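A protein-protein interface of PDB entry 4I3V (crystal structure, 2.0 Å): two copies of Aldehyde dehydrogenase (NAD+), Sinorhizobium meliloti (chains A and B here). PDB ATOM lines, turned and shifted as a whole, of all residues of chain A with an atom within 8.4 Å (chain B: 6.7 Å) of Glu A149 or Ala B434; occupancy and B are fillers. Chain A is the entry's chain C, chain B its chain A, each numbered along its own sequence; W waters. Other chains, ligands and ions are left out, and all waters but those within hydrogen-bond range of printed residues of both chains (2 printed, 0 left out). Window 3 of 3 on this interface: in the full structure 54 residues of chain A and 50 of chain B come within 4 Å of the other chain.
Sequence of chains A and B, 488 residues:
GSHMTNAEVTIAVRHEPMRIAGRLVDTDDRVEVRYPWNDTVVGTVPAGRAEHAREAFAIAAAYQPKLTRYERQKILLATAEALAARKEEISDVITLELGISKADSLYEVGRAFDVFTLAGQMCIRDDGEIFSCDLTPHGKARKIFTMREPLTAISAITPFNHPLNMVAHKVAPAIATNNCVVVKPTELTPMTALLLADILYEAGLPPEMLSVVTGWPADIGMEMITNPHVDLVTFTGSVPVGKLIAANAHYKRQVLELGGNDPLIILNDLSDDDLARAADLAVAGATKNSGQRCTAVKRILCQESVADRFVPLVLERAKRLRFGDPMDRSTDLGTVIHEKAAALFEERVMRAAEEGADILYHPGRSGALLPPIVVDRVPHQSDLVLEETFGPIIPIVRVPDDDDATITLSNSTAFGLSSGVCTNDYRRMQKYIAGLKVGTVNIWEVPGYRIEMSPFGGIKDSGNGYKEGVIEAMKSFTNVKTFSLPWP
The backbone carbonyl oxygen (O) of Ile B433 lies within hydrogen-bond range of the side-chain amino group (NZ) of Lys A481 (2.8 Å). NZ of Lys A481 lies within hydrogen-bond range of O of Ala B434 (3.2 Å). NZ of Lys A481 sits at hydrogen-bond distance from O of Leu B436. The backbone NH (N) of Val B441 lies within hydrogen-bond range of the backbone carbonyl oxygen (O) of Thr A482 (2.9 Å).
The backbone carbonyl oxygen (O) of Met A147 lies within hydrogen-bond range of the backbone NH (N) of Lys A481 (2.7 Å). The backbone NH (N) of Asn A479 sits at hydrogen-bond distance from the backbone carbonyl oxygen (O) of Glu A149 (2.7 Å). The side-chain amino group (NZ) of Lys A481 is in salt-bridge range of the side-chain carboxylate (OE2) of Glu A149 (2.7 Å). NH2 of Arg A253 is in hydrogen-bond range of OD1 of Asn A479.
Among the printed residues, merely in contact across the chains: Glu A149 with Ala B434, Asn A479 with Ile B459, Lys A481 with Val B438, Phe A483 with Ile B433 and Phe A483 with Val B441.
Of chain B, only Ala B434 comes within 4 Å of Glu A149. Of the printed residues of chain B, Asn A479 touches Ile B459. Of the printed residues of chain B, Phe A483 touches Ile B433 and Val B441. Of the printed residues of chain A, Ile B433 touches Lys A481 (2.8 Å) and Phe A483 (3.5 Å). Ala B434 touches just these residues of chain A: Glu A149 and Lys A481. Of the printed residues of chain A, Ile B459 touches Asn A479 (3.5 Å). The nearest printed residue of chain A that does not touch Ile B459 is Arg A253 (5.9 Å).
Hydrophobic or aromatic side chains of chain B within 4 Å of the printed part of chain A: Ile B433 and Ile B459. Of the 23 printed residues of chain A, 5 touch a printed residue of chain B. Hydrophobic or aromatic side chains of chain A within 4 Å of the printed part of chain B: Phe A483. Among the printed residues, no Asp or Glu carboxylate lies within 4 Å of a Lys or Arg side-chain nitrogen of the other chain.
No position is printed for both chains.
Water W2 bridges OE2 of Glu A149 (2.5 Å) and O of Ala B434 (3.5 Å). Water W1 lies within hydrogen-bond range of O of Ala B434 (2.9 Å) and OE1 of Glu A149 (3.4 Å).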
ATOM      1  N   ARG A  69       7.047 -30.695  25.292  1.00  0.00           N
ATOM      2  CA  ARG A  69       6.068 -30.465  26.356  1.00  0.00           C
ATOM      3  C   ARG A  69       6.684 -30.678  27.740  1.00  0.00           C
ATOM      4  O   ARG A  69       6.373 -29.954  28.698  1.00  0.00           O
ATOM      5  CB  ARG A  69       4.836 -31.346  26.155  1.00  0.00           C
ATOM      6  CG  ARG A  69       4.068 -30.994  24.875  1.00  0.00           C
ATOM      7  CD  ARG A  69       2.974 -32.006  24.567  1.00  0.00           C
ATOM      8  NE  ARG A  69       2.104 -31.592  23.464  1.00  0.00           N
ATOM      9  CZ  ARG A  69       0.896 -31.048  23.615  1.00  0.00           C
ATOM     10  NH1 ARG A  69       0.404 -30.816  24.827  1.00  0.00           N
ATOM     11  NH2 ARG A  69       0.175 -30.734  22.549  1.00  0.00           N
ATOM     12  N   THR A 146      -6.637 -33.216  13.957  1.00  0.00           N
ATOM     13  CA  THR A 146      -6.540 -31.835  14.381  1.00  0.00           C
ATOM     14  C   THR A 146      -5.290 -31.602  15.264  1.00  0.00           C
ATOM     15  O   THR A 146      -4.939 -32.441  16.097  1.00  0.00           O
ATOM     16  CB  THR A 146      -7.850 -31.510  15.110  1.00  0.00           C
ATOM     17  OG1 THR A 146      -8.633 -30.587  14.338  1.00  0.00           O
ATOM     18  CG2 THR A 146      -7.600 -31.024  16.463  1.00  0.00           C
ATOM     19  N   MET A 147      -4.633 -30.459  15.082  1.00  0.00           N
ATOM     20  CA  MET A 147      -3.313 -30.192  15.648  1.00  0.00           C
ATOM     21  C   MET A 147      -3.276 -28.711  16.029  1.00  0.00           C
ATOM     22  O   MET A 147      -3.929 -27.914  15.374  1.00  0.00           O
ATOM     23  CB  MET A 147      -2.293 -30.409  14.524  1.00  0.00           C
ATOM     24  CG  MET A 147      -1.086 -31.195  14.864  1.00  0.00           C
ATOM     25  SD  MET A 147       0.087 -31.055  13.494  1.00  0.00           S
ATOM     26  CE  MET A 147       0.951 -29.544  13.936  1.00  0.00           C
ATOM     27  N   ARG A 148      -2.514 -28.338  17.055  1.00  0.00           N
ATOM     28  CA  ARG A 148      -2.329 -26.914  17.390  1.00  0.00           C
ATOM     29  C   ARG A 148      -0.901 -26.440  17.167  1.00  0.00           C
ATOM     30  O   ARG A 148       0.036 -27.177  17.439  1.00  0.00           O
ATOM     31  CB  ARG A 148      -2.704 -26.630  18.846  1.00  0.00           C
ATOM     32  CG  ARG A 148      -4.190 -26.574  19.099  1.00  0.00           C
ATOM     33  CD  ARG A 148      -4.503 -26.355  20.589  1.00  0.00           C
ATOM     34  NE  ARG A 148      -5.931 -26.531  20.795  1.00  0.00           N
ATOM     35  CZ  ARG A 148      -6.847 -25.635  20.447  1.00  0.00           C
ATOM     36  NH1 ARG A 148      -6.481 -24.467  19.926  1.00  0.00           N
ATOM     37  NH2 ARG A 148      -8.130 -25.893  20.666  1.00  0.00           N
ATOM     38  N   GLU A 149      -0.747 -25.202  16.702  1.00  0.00           N
ATOM     39  CA  GLU A 149       0.564 -24.609  16.451  1.00  0.00           C
ATOM     40  C   GLU A 149       0.599 -23.196  17.029  1.00  0.00           C
ATOM     41  O   GLU A 149      -0.423 -22.522  17.078  1.00  0.00           O
ATOM     42  CB  GLU A 149       0.857 -24.542  14.944  1.00  0.00           C
ATOM     43  CG  GLU A 149       1.082 -25.904  14.263  1.00  0.00           C
ATOM     44  CD  GLU A 149       1.399 -25.765  12.763  1.00  0.00           C
ATOM     45  OE1 GLU A 149       1.249 -24.647  12.219  1.00  0.00           O
ATOM     46  OE2 GLU A 149       1.790 -26.768  12.129  1.00  0.00           O
ATOM     47  N   PRO A 150       1.782 -22.734  17.444  1.00  0.00           N
ATOM     48  CA  PRO A 150       1.860 -21.401  18.045  1.00  0.00           C
ATOM     49  C   PRO A 150       1.819 -20.267  17.025  1.00  0.00           C
ATOM     50  O   PRO A 150       1.925 -20.476  15.817  1.00  0.00           O
ATOM     51  CB  PRO A 150       3.213 -21.420  18.748  1.00  0.00           C
ATOM     52  CG  PRO A 150       4.027 -22.428  17.986  1.00  0.00           C
ATOM     53  CD  PRO A 150       3.046 -23.482  17.576  1.00  0.00           C
ATOM     54  N   LEU A 151       1.678 -19.054  17.536  1.00  0.00           N
ATOM     55  CA  LEU A 151       1.675 -17.857  16.709  1.00  0.00           C
ATOM     56  C   LEU A 151       3.094 -17.307  16.594  1.00  0.00           C
ATOM     57  O   LEU A 151       4.017 -17.840  17.186  1.00  0.00           O
ATOM     58  CB  LEU A 151       0.753 -16.802  17.330  1.00  0.00           C
ATOM     59  CG  LEU A 151      -0.526 -17.357  17.967  1.00  0.00           C
ATOM     60  CD1 LEU A 151      -1.338 -16.252  18.693  1.00  0.00           C
ATOM     61  CD2 LEU A 151      -1.397 -18.064  16.951  1.00  0.00           C
ATOM     62  N   THR A 152       3.254 -16.236  15.827  1.00  0.00           N
ATOM     63  CA  THR A 152       4.552 -15.624  15.606  1.00  0.00           C
ATOM     64  C   THR A 152       5.023 -14.873  16.861  1.00  0.00           C
ATOM     65  O   THR A 152       6.149 -15.062  17.337  1.00  0.00           O
ATOM     66  CB  THR A 152       4.496 -14.665  14.388  1.00  0.00           C
ATOM     67  OG1 THR A 152       4.180 -15.415  13.200  1.00  0.00           O
ATOM     68  CG2 THR A 152       5.824 -13.937  14.203  1.00  0.00           C
ATOM     69  N   THR A 177       2.598 -22.975  25.359  1.00  0.00           N
ATOM     70  CA  THR A 177       2.244 -23.230  23.955  1.00  0.00           C
ATOM     71  C   THR A 177       3.371 -22.959  22.966  1.00  0.00           C
ATOM     72  O   THR A 177       3.136 -22.924  21.760  1.00  0.00           O
ATOM     73  CB  THR A 177       1.031 -22.364  23.495  1.00  0.00           C
ATOM     74  OG1 THR A 177       1.139 -21.042  24.034  1.00  0.00           O
ATOM     75  CG2 THR A 177      -0.247 -22.942  23.975  1.00  0.00           C
ATOM     76  N   ASN A 178       4.584 -22.734  23.465  1.00  0.00           N
ATOM     77  CA  ASN A 178       5.719 -22.420  22.587  1.00  0.00           C
ATOM     78  C   ASN A 178       5.539 -21.121  21.805  1.00  0.00           C
ATOM     79  O   ASN A 178       5.982 -20.999  20.666  1.00  0.00           O
ATOM     80  CB  ASN A 178       6.077 -23.588  21.649  1.00  0.00           C
ATOM     81  CG  ASN A 178       7.141 -24.515  22.241  1.00  0.00           C
ATOM     82  OD1 ASN A 178       7.784 -24.170  23.223  1.00  0.00           O
ATOM     83  ND2 ASN A 178       7.340 -25.678  21.631  1.00  0.00           N
ATOM     84  N   ASN A 179       4.884 -20.150  22.426  1.00  0.00           N
ATOM     85  CA  ASN A 179       4.810 -18.807  21.868  1.00  0.00           C
ATOM     86  C   ASN A 179       5.929 -17.922  22.414  1.00  0.00           C
ATOM     87  O   ASN A 179       6.619 -18.296  23.361  1.00  0.00           O
ATOM     88  CB  ASN A 179       3.455 -18.174  22.185  1.00  0.00           C
ATOM     89  CG  ASN A 179       2.382 -18.614  21.229  1.00  0.00           C
ATOM     90  OD1 ASN A 179       2.341 -18.160  20.078  1.00  0.00           O
ATOM     91  ND2 ASN A 179       1.507 -19.532  21.686  1.00  0.00           N
ATOM     92  N   ASP A 231       0.554 -11.349  16.262  1.00  0.00           N
ATOM     93  CA  ASP A 231      -0.600 -12.127  15.825  1.00  0.00           C
ATOM     94  C   ASP A 231      -1.793 -11.949  16.780  1.00  0.00           C
ATOM     95  O   ASP A 231      -2.936 -12.144  16.396  1.00  0.00           O
ATOM     96  CB  ASP A 231      -0.233 -13.616  15.719  1.00  0.00           C
ATOM     97  CG  ASP A 231       0.562 -13.944  14.456  1.00  0.00           C
ATOM     98  OD1 ASP A 231       0.711 -13.055  13.588  1.00  0.00           O
ATOM     99  OD2 ASP A 231       1.029 -15.096  14.325  1.00  0.00           O
ATOM    100  N   ARG A 253      -5.993 -10.050  15.939  1.00  0.00           N
ATOM    101  CA  ARG A 253      -6.756 -10.776  16.950  1.00  0.00           C
ATOM    102  C   ARG A 253      -6.551 -10.119  18.304  1.00  0.00           C
ATOM    103  O   ARG A 253      -5.437  -9.723  18.647  1.00  0.00           O
ATOM    104  CB  ARG A 253      -6.304 -12.236  17.049  1.00  0.00           C
ATOM    105  CG  ARG A 253      -7.181 -13.219  16.305  1.00  0.00           C
ATOM    106  CD  ARG A 253      -7.146 -14.626  16.921  1.00  0.00           C
ATOM    107  NE  ARG A 253      -6.035 -15.517  16.536  1.00  0.00           N
ATOM    108  CZ  ARG A 253      -5.291 -15.437  15.421  1.00  0.00           C
ATOM    109  NH1 ARG A 253      -5.499 -14.470  14.524  1.00  0.00           N
ATOM    110  NH2 ARG A 253      -4.324 -16.342  15.191  1.00  0.00           N
ATOM    111  N   MET A 474      -4.514 -20.817  26.605  1.00  0.00           N
ATOM    112  CA  MET A 474      -3.707 -21.750  25.836  1.00  0.00           C
ATOM    113  C   MET A 474      -4.313 -21.992  24.453  1.00  0.00           C
ATOM    114  O   MET A 474      -3.611 -22.000  23.450  1.00  0.00           O
ATOM    115  CB  MET A 474      -3.519 -23.075  26.592  1.00  0.00           C
ATOM    116  CG  MET A 474      -2.409 -22.984  27.652  1.00  0.00           C
ATOM    117  SD  MET A 474      -2.244 -24.451  28.668  1.00  0.00           S
ATOM    118  CE  MET A 474      -1.393 -25.603  27.593  1.00  0.00           C
ATOM    119  N   LYS A 475      -5.624 -22.188  24.402  1.00  0.00           N
ATOM    120  CA  LYS A 475      -6.272 -22.405  23.121  1.00  0.00           C
ATOM    121  C   LYS A 475      -6.237 -21.149  22.239  1.00  0.00           C
ATOM    122  O   LYS A 475      -5.914 -21.231  21.054  1.00  0.00           O
ATOM    123  CB  LYS A 475      -7.684 -22.932  23.324  1.00  0.00           C
ATOM    124  CG  LYS A 475      -7.676 -24.182  24.196  1.00  0.00           C
ATOM    125  CD  LYS A 475      -8.644 -25.234  23.735  1.00  0.00           C
ATOM    126  CE  LYS A 475      -9.914 -25.174  24.536  1.00  0.00           C
ATOM    127  NZ  LYS A 475     -10.663 -23.948  24.185  1.00  0.00           N
ATOM    128  N   SER A 476      -6.524 -19.986  22.819  1.00  0.00           N
ATOM    129  CA  SER A 476      -6.542 -18.757  22.021  1.00  0.00           C
ATOM    130  C   SER A 476      -5.160 -18.413  21.475  1.00  0.00           C
ATOM    131  O   SER A 476      -5.045 -17.678  20.494  1.00  0.00           O
ATOM    132  CB  SER A 476      -7.082 -17.574  22.839  1.00  0.00           C
ATOM    133  OG  SER A 476      -6.087 -17.113  23.731  1.00  0.00           O
ATOM    134  N   PHE A 477      -4.113 -18.939  22.117  1.00  0.00           N
ATOM    135  CA  PHE A 477      -2.736 -18.583  21.792  1.00  0.00           C
ATOM    136  C   PHE A 477      -2.173 -19.519  20.716  1.00  0.00           C
ATOM    137  O   PHE A 477      -0.973 -19.536  20.469  1.00  0.00           O
ATOM    138  CB  PHE A 477      -1.832 -18.660  23.036  1.00  0.00           C
ATOM    139  CG  PHE A 477      -2.011 -17.517  24.034  1.00  0.00           C
ATOM    140  CD1 PHE A 477      -3.005 -16.566  23.880  1.00  0.00           C
ATOM    141  CD2 PHE A 477      -1.163 -17.414  25.131  1.00  0.00           C
ATOM    142  CE1 PHE A 477      -3.151 -15.525  24.809  1.00  0.00           C
ATOM    143  CE2 PHE A 477      -1.296 -16.369  26.056  1.00  0.00           C
ATOM    144  CZ  PHE A 477      -2.298 -15.437  25.897  1.00  0.00           C
ATOM    145  N   THR A 478      -3.036 -20.321  20.106  1.00  0.00           N
ATOM    146  CA  THR A 478      -2.607 -21.225  19.040  1.00  0.00           C
ATOM    147  C   THR A 478      -3.483 -21.120  17.783  1.00  0.00           C
ATOM    148  O   THR A 478      -4.586 -20.572  17.808  1.00  0.00           O
ATOM    149  CB  THR A 478      -2.590 -22.709  19.504  1.00  0.00           C
ATOM    150  OG1 THR A 478      -3.896 -23.089  19.936  1.00  0.00           O
ATOM    151  CG2 THR A 478      -1.610 -22.929  20.649  1.00  0.00           C
ATOM    152  N   ASN A 479      -2.963 -21.633  16.678  1.00  0.00           N
ATOM    153  CA  ASN A 479      -3.763 -21.863  15.482  1.00  0.00           C
ATOM    154  C   ASN A 479      -3.998 -23.353  15.387  1.00  0.00           C
ATOM    155  O   ASN A 479      -3.076 -24.150  15.596  1.00  0.00           O
ATOM    156  CB  ASN A 479      -3.042 -21.379  14.224  1.00  0.00           C
ATOM    157  CG  ASN A 479      -2.981 -19.859  14.127  1.00  0.00           C
ATOM    158  OD1 ASN A 479      -3.938 -19.172  14.450  1.00  0.00           O
ATOM    159  ND2 ASN A 479      -1.864 -19.342  13.659  1.00  0.00           N
ATOM    160  N   VAL A 480      -5.226 -23.730  15.081  1.00  0.00           N
ATOM    161  CA  VAL A 480      -5.546 -25.126  14.839  1.00  0.00           C
ATOM    162  C   VAL A 480      -5.264 -25.466  13.380  1.00  0.00           C
ATOM    163  O   VAL A 480      -5.793 -24.822  12.475  1.00  0.00           O
ATOM    164  CB  VAL A 480      -7.020 -25.421  15.177  1.00  0.00           C
ATOM    165  CG1 VAL A 480      -7.425 -26.795  14.667  1.00  0.00           C
ATOM    166  CG2 VAL A 480      -7.249 -25.305  16.697  1.00  0.00           C
ATOM    167  N   LYS A 481      -4.400 -26.454  13.156  1.00  0.00           N
ATOM    168  CA  LYS A 481      -4.201 -27.000  11.818  1.00  0.00           C
ATOM    169  C   LYS A 481      -4.941 -28.330  11.708  1.00  0.00           C
ATOM    170  O   LYS A 481      -4.904 -29.149  12.629  1.00  0.00           O
ATOM    171  CB  LYS A 481      -2.708 -27.204  11.518  1.00  0.00           C
ATOM    172  CG  LYS A 481      -2.412 -27.781  10.127  1.00  0.00           C
ATOM    173  CD  LYS A 481      -0.893 -27.996   9.897  1.00  0.00           C
ATOM    174  CE  LYS A 481      -0.175 -26.682   9.545  1.00  0.00           C
ATOM    175  NZ  LYS A 481       1.329 -26.807   9.493  1.00  0.00           N
ATOM    176  N   THR A 482      -5.626 -28.555  10.596  1.00  0.00           N
ATOM    177  CA  THR A 482      -6.151 -29.893  10.367  1.00  0.00           C
ATOM    178  C   THR A 482      -5.361 -30.589   9.255  1.00  0.00           C
ATOM    179  O   THR A 482      -4.753 -29.940   8.389  1.00  0.00           O
ATOM    180  CB  THR A 482      -7.654 -29.873  10.001  1.00  0.00           C
ATOM    181  OG1 THR A 482      -7.803 -29.525   8.620  1.00  0.00           O
ATOM    182  CG2 THR A 482      -8.406 -28.868  10.879  1.00  0.00           C
ATOM    183  N   PHE A 483      -5.345 -31.911   9.289  1.00  0.00           N
ATOM    184  CA  PHE A 483      -4.861 -32.661   8.134  1.00  0.00           C
ATOM    185  C   PHE A 483      -5.713 -33.907   7.955  1.00  0.00           C
ATOM    186  O   PHE A 483      -6.318 -34.394   8.916  1.00  0.00           O
ATOM    187  CB  PHE A 483      -3.367 -32.993   8.237  1.00  0.00           C
ATOM    188  CG  PHE A 483      -3.006 -33.841   9.413  1.00  0.00           C
ATOM    189  CD1 PHE A 483      -2.778 -33.268  10.655  1.00  0.00           C
ATOM    190  CD2 PHE A 483      -2.874 -35.220   9.275  1.00  0.00           C
ATOM    191  CE1 PHE A 483      -2.423 -34.052  11.748  1.00  0.00           C
ATOM    192  CE2 PHE A 483      -2.531 -36.018  10.361  1.00  0.00           C
ATOM    193  CZ  PHE A 483      -2.296 -35.428  11.604  1.00  0.00           C
ATOM    194  N   MET B 429       5.184 -36.775   3.786  1.00  0.00           N
ATOM    195  CA  MET B 429       3.839 -36.389   4.211  1.00  0.00           C
ATOM    196  C   MET B 429       3.862 -35.592   5.505  1.00  0.00           C
ATOM    197  O   MET B 429       3.242 -34.535   5.578  1.00  0.00           O
ATOM    198  CB  MET B 429       2.996 -37.634   4.476  1.00  0.00           C
ATOM    199  CG  MET B 429       2.045 -38.027   3.404  1.00  0.00           C
ATOM    200  SD  MET B 429       1.196 -39.547   3.884  1.00  0.00           S
ATOM    201  CE  MET B 429       0.855 -40.206   2.241  1.00  0.00           C
ATOM    202  N   GLN B 430       4.514 -36.155   6.528  1.00  0.00           N
ATOM    203  CA  GLN B 430       4.723 -35.501   7.838  1.00  0.00           C
ATOM    204  C   GLN B 430       5.348 -34.136   7.673  1.00  0.00           C
ATOM    205  O   GLN B 430       4.944 -33.151   8.313  1.00  0.00           O
ATOM    206  CB  GLN B 430       5.700 -36.314   8.710  1.00  0.00           C
ATOM    207  CG  GLN B 430       6.578 -35.377   9.690  1.00  0.00           C
ATOM    208  CD  GLN B 430       5.732 -35.053  10.856  1.00  0.00           C
ATOM    209  OE1 GLN B 430       4.647 -35.611  10.950  1.00  0.00           O
ATOM    210  NE2 GLN B 430       6.180 -34.188  11.752  1.00  0.00           N
ATOM    211  N   LYS B 431       6.378 -34.100   6.834  1.00  0.00           N
ATOM    212  CA  LYS B 431       7.156 -32.890   6.626  1.00  0.00           C
ATOM    213  C   LYS B 431       6.271 -31.771   6.086  1.00  0.00           C
ATOM    214  O   LYS B 431       6.363 -30.639   6.547  1.00  0.00           O
ATOM    215  CB  LYS B 431       8.328 -33.161   5.660  1.00  0.00           C
ATOM    216  CG  LYS B 431       9.340 -32.003   5.514  1.00  0.00           C
ATOM    217  CD  LYS B 431      10.530 -32.430   4.655  1.00  0.00           C
ATOM    218  CE  LYS B 431      11.437 -31.275   4.300  1.00  0.00           C
ATOM    219  NZ  LYS B 431      12.147 -30.721   5.488  1.00  0.00           N
ATOM    220  N   TYR B 432       5.424 -32.095   5.107  1.00  0.00           N
ATOM    221  CA  TYR B 432       4.547 -31.097   4.487  1.00  0.00           C
ATOM    222  C   TYR B 432       3.429 -30.706   5.460  1.00  0.00           C
ATOM    223  O   TYR B 432       3.097 -29.531   5.615  1.00  0.00           O
ATOM    224  CB  TYR B 432       3.973 -31.620   3.148  1.00  0.00           C
ATOM    225  CG  TYR B 432       4.933 -31.435   2.001  1.00  0.00           C
ATOM    226  CD1 TYR B 432       5.949 -32.354   1.773  1.00  0.00           C
ATOM    227  CD2 TYR B 432       4.856 -30.317   1.169  1.00  0.00           C
ATOM    228  CE1 TYR B 432       6.854 -32.184   0.748  1.00  0.00           C
ATOM    229  CE2 TYR B 432       5.762 -30.138   0.127  1.00  0.00           C
ATOM    230  CZ  TYR B 432       6.765 -31.082  -0.072  1.00  0.00           C
ATOM    231  OH  TYR B 432       7.685 -30.930  -1.095  1.00  0.00           O
ATOM    232  N   ILE B 433       2.851 -31.697   6.122  1.00  0.00           N
ATOM    233  CA  ILE B 433       1.796 -31.415   7.098  1.00  0.00           C
ATOM    234  C   ILE B 433       2.340 -30.425   8.131  1.00  0.00           C
ATOM    235  O   ILE B 433       1.703 -29.403   8.438  1.00  0.00           O
ATOM    236  CB  ILE B 433       1.280 -32.718   7.760  1.00  0.00           C
ATOM    237  CG1 ILE B 433       0.530 -33.579   6.734  1.00  0.00           C
ATOM    238  CG2 ILE B 433       0.377 -32.417   8.960  1.00  0.00           C
ATOM    239  CD1 ILE B 433       0.041 -34.906   7.290  1.00  0.00           C
ATOM    240  N   ALA B 434       3.543 -30.691   8.625  1.00  0.00           N
ATOM    241  CA  ALA B 434       4.132 -29.835   9.655  1.00  0.00           C
ATOM    242  C   ALA B 434       4.586 -28.487   9.116  1.00  0.00           C
ATOM    243  O   ALA B 434       4.476 -27.480   9.814  1.00  0.00           O
ATOM    244  CB  ALA B 434       5.302 -30.539  10.354  1.00  0.00           C
ATOM    245  N   GLY B 435       5.089 -28.467   7.880  1.00  0.00           N
ATOM    246  CA  GLY B 435       5.788 -27.299   7.369  1.00  0.00           C
ATOM    247  C   GLY B 435       4.974 -26.322   6.535  1.00  0.00           C
ATOM    248  O   GLY B 435       5.394 -25.191   6.322  1.00  0.00           O
ATOM    249  N   LEU B 436       3.817 -26.739   6.044  1.00  0.00           N
ATOM    250  CA  LEU B 436       3.021 -25.819   5.245  1.00  0.00           C
ATOM    251  C   LEU B 436       2.284 -24.842   6.165  1.00  0.00           C
ATOM    252  O   LEU B 436       1.637 -25.233   7.154  1.00  0.00           O
ATOM    253  CB  LEU B 436       2.064 -26.565   4.297  1.00  0.00           C
ATOM    254  CG  LEU B 436       2.696 -27.389   3.154  1.00  0.00           C
ATOM    255  CD1 LEU B 436       1.641 -28.302   2.511  1.00  0.00           C
ATOM    256  CD2 LEU B 436       3.312 -26.499   2.091  1.00  0.00           C
ATOM    257  N   LYS B 437       2.403 -23.560   5.852  1.00  0.00           N
ATOM    258  CA  LYS B 437       1.765 -22.540   6.687  1.00  0.00           C
ATOM    259  C   LYS B 437       0.326 -22.299   6.230  1.00  0.00           C
ATOM    260  O   LYS B 437       0.045 -21.339   5.515  1.00  0.00           O
ATOM    261  CB  LYS B 437       2.590 -21.251   6.674  1.00  0.00           C
ATOM    262  CG  LYS B 437       3.993 -21.407   7.234  1.00  0.00           C
ATOM    263  CD  LYS B 437       4.755 -20.090   7.164  1.00  0.00           C
ATOM    264  CE  LYS B 437       6.267 -20.279   7.318  1.00  0.00           C
ATOM    265  NZ  LYS B 437       6.689 -20.307   8.748  1.00  0.00           N
ATOM    266  N   VAL B 438      -0.569 -23.201   6.629  1.00  0.00           N
ATOM    267  CA  VAL B 438      -1.963 -23.174   6.196  1.00  0.00           C
ATOM    268  C   VAL B 438      -2.834 -23.688   7.330  1.00  0.00           C
ATOM    269  O   VAL B 438      -2.321 -24.191   8.330  1.00  0.00           O
ATOM    270  CB  VAL B 438      -2.187 -24.090   4.945  1.00  0.00           C
ATOM    271  CG1 VAL B 438      -1.432 -23.538   3.724  1.00  0.00           C
ATOM    272  CG2 VAL B 438      -1.762 -25.526   5.239  1.00  0.00           C
ATOM    273  N   VAL B 441      -4.055 -29.329   5.613  1.00  0.00           N
ATOM    274  CA  VAL B 441      -3.232 -30.046   4.644  1.00  0.00           C
ATOM    275  C   VAL B 441      -3.937 -31.358   4.287  1.00  0.00           C
ATOM    276  O   VAL B 441      -4.063 -32.245   5.129  1.00  0.00           O
ATOM    277  CB  VAL B 441      -1.805 -30.357   5.167  1.00  0.00           C
ATOM    278  CG1 VAL B 441      -1.008 -31.085   4.089  1.00  0.00           C
ATOM    279  CG2 VAL B 441      -1.061 -29.064   5.609  1.00  0.00           C
ATOM    280  N   ILE B 459      -4.825 -18.924   7.913  1.00  0.00           N
ATOM    281  CA  ILE B 459      -3.986 -17.959   8.618  1.00  0.00           C
ATOM    282  C   ILE B 459      -3.494 -16.921   7.625  1.00  0.00           C
ATOM    283  O   ILE B 459      -3.904 -16.930   6.465  1.00  0.00           O
ATOM    284  CB  ILE B 459      -2.785 -18.660   9.298  1.00  0.00           C
ATOM    285  CG1 ILE B 459      -1.991 -19.470   8.263  1.00  0.00           C
ATOM    286  CG2 ILE B 459      -3.274 -19.588  10.426  1.00  0.00           C
ATOM    287  CD1 ILE B 459      -0.738 -20.147   8.810  1.00  0.00           C
HETATM  288  O   HOH W   1       3.971 -24.619  10.209  1.00  0.00           O
HETATM  289  O   HOH W   2       3.640 -28.041  13.121  1.00  0.00           O
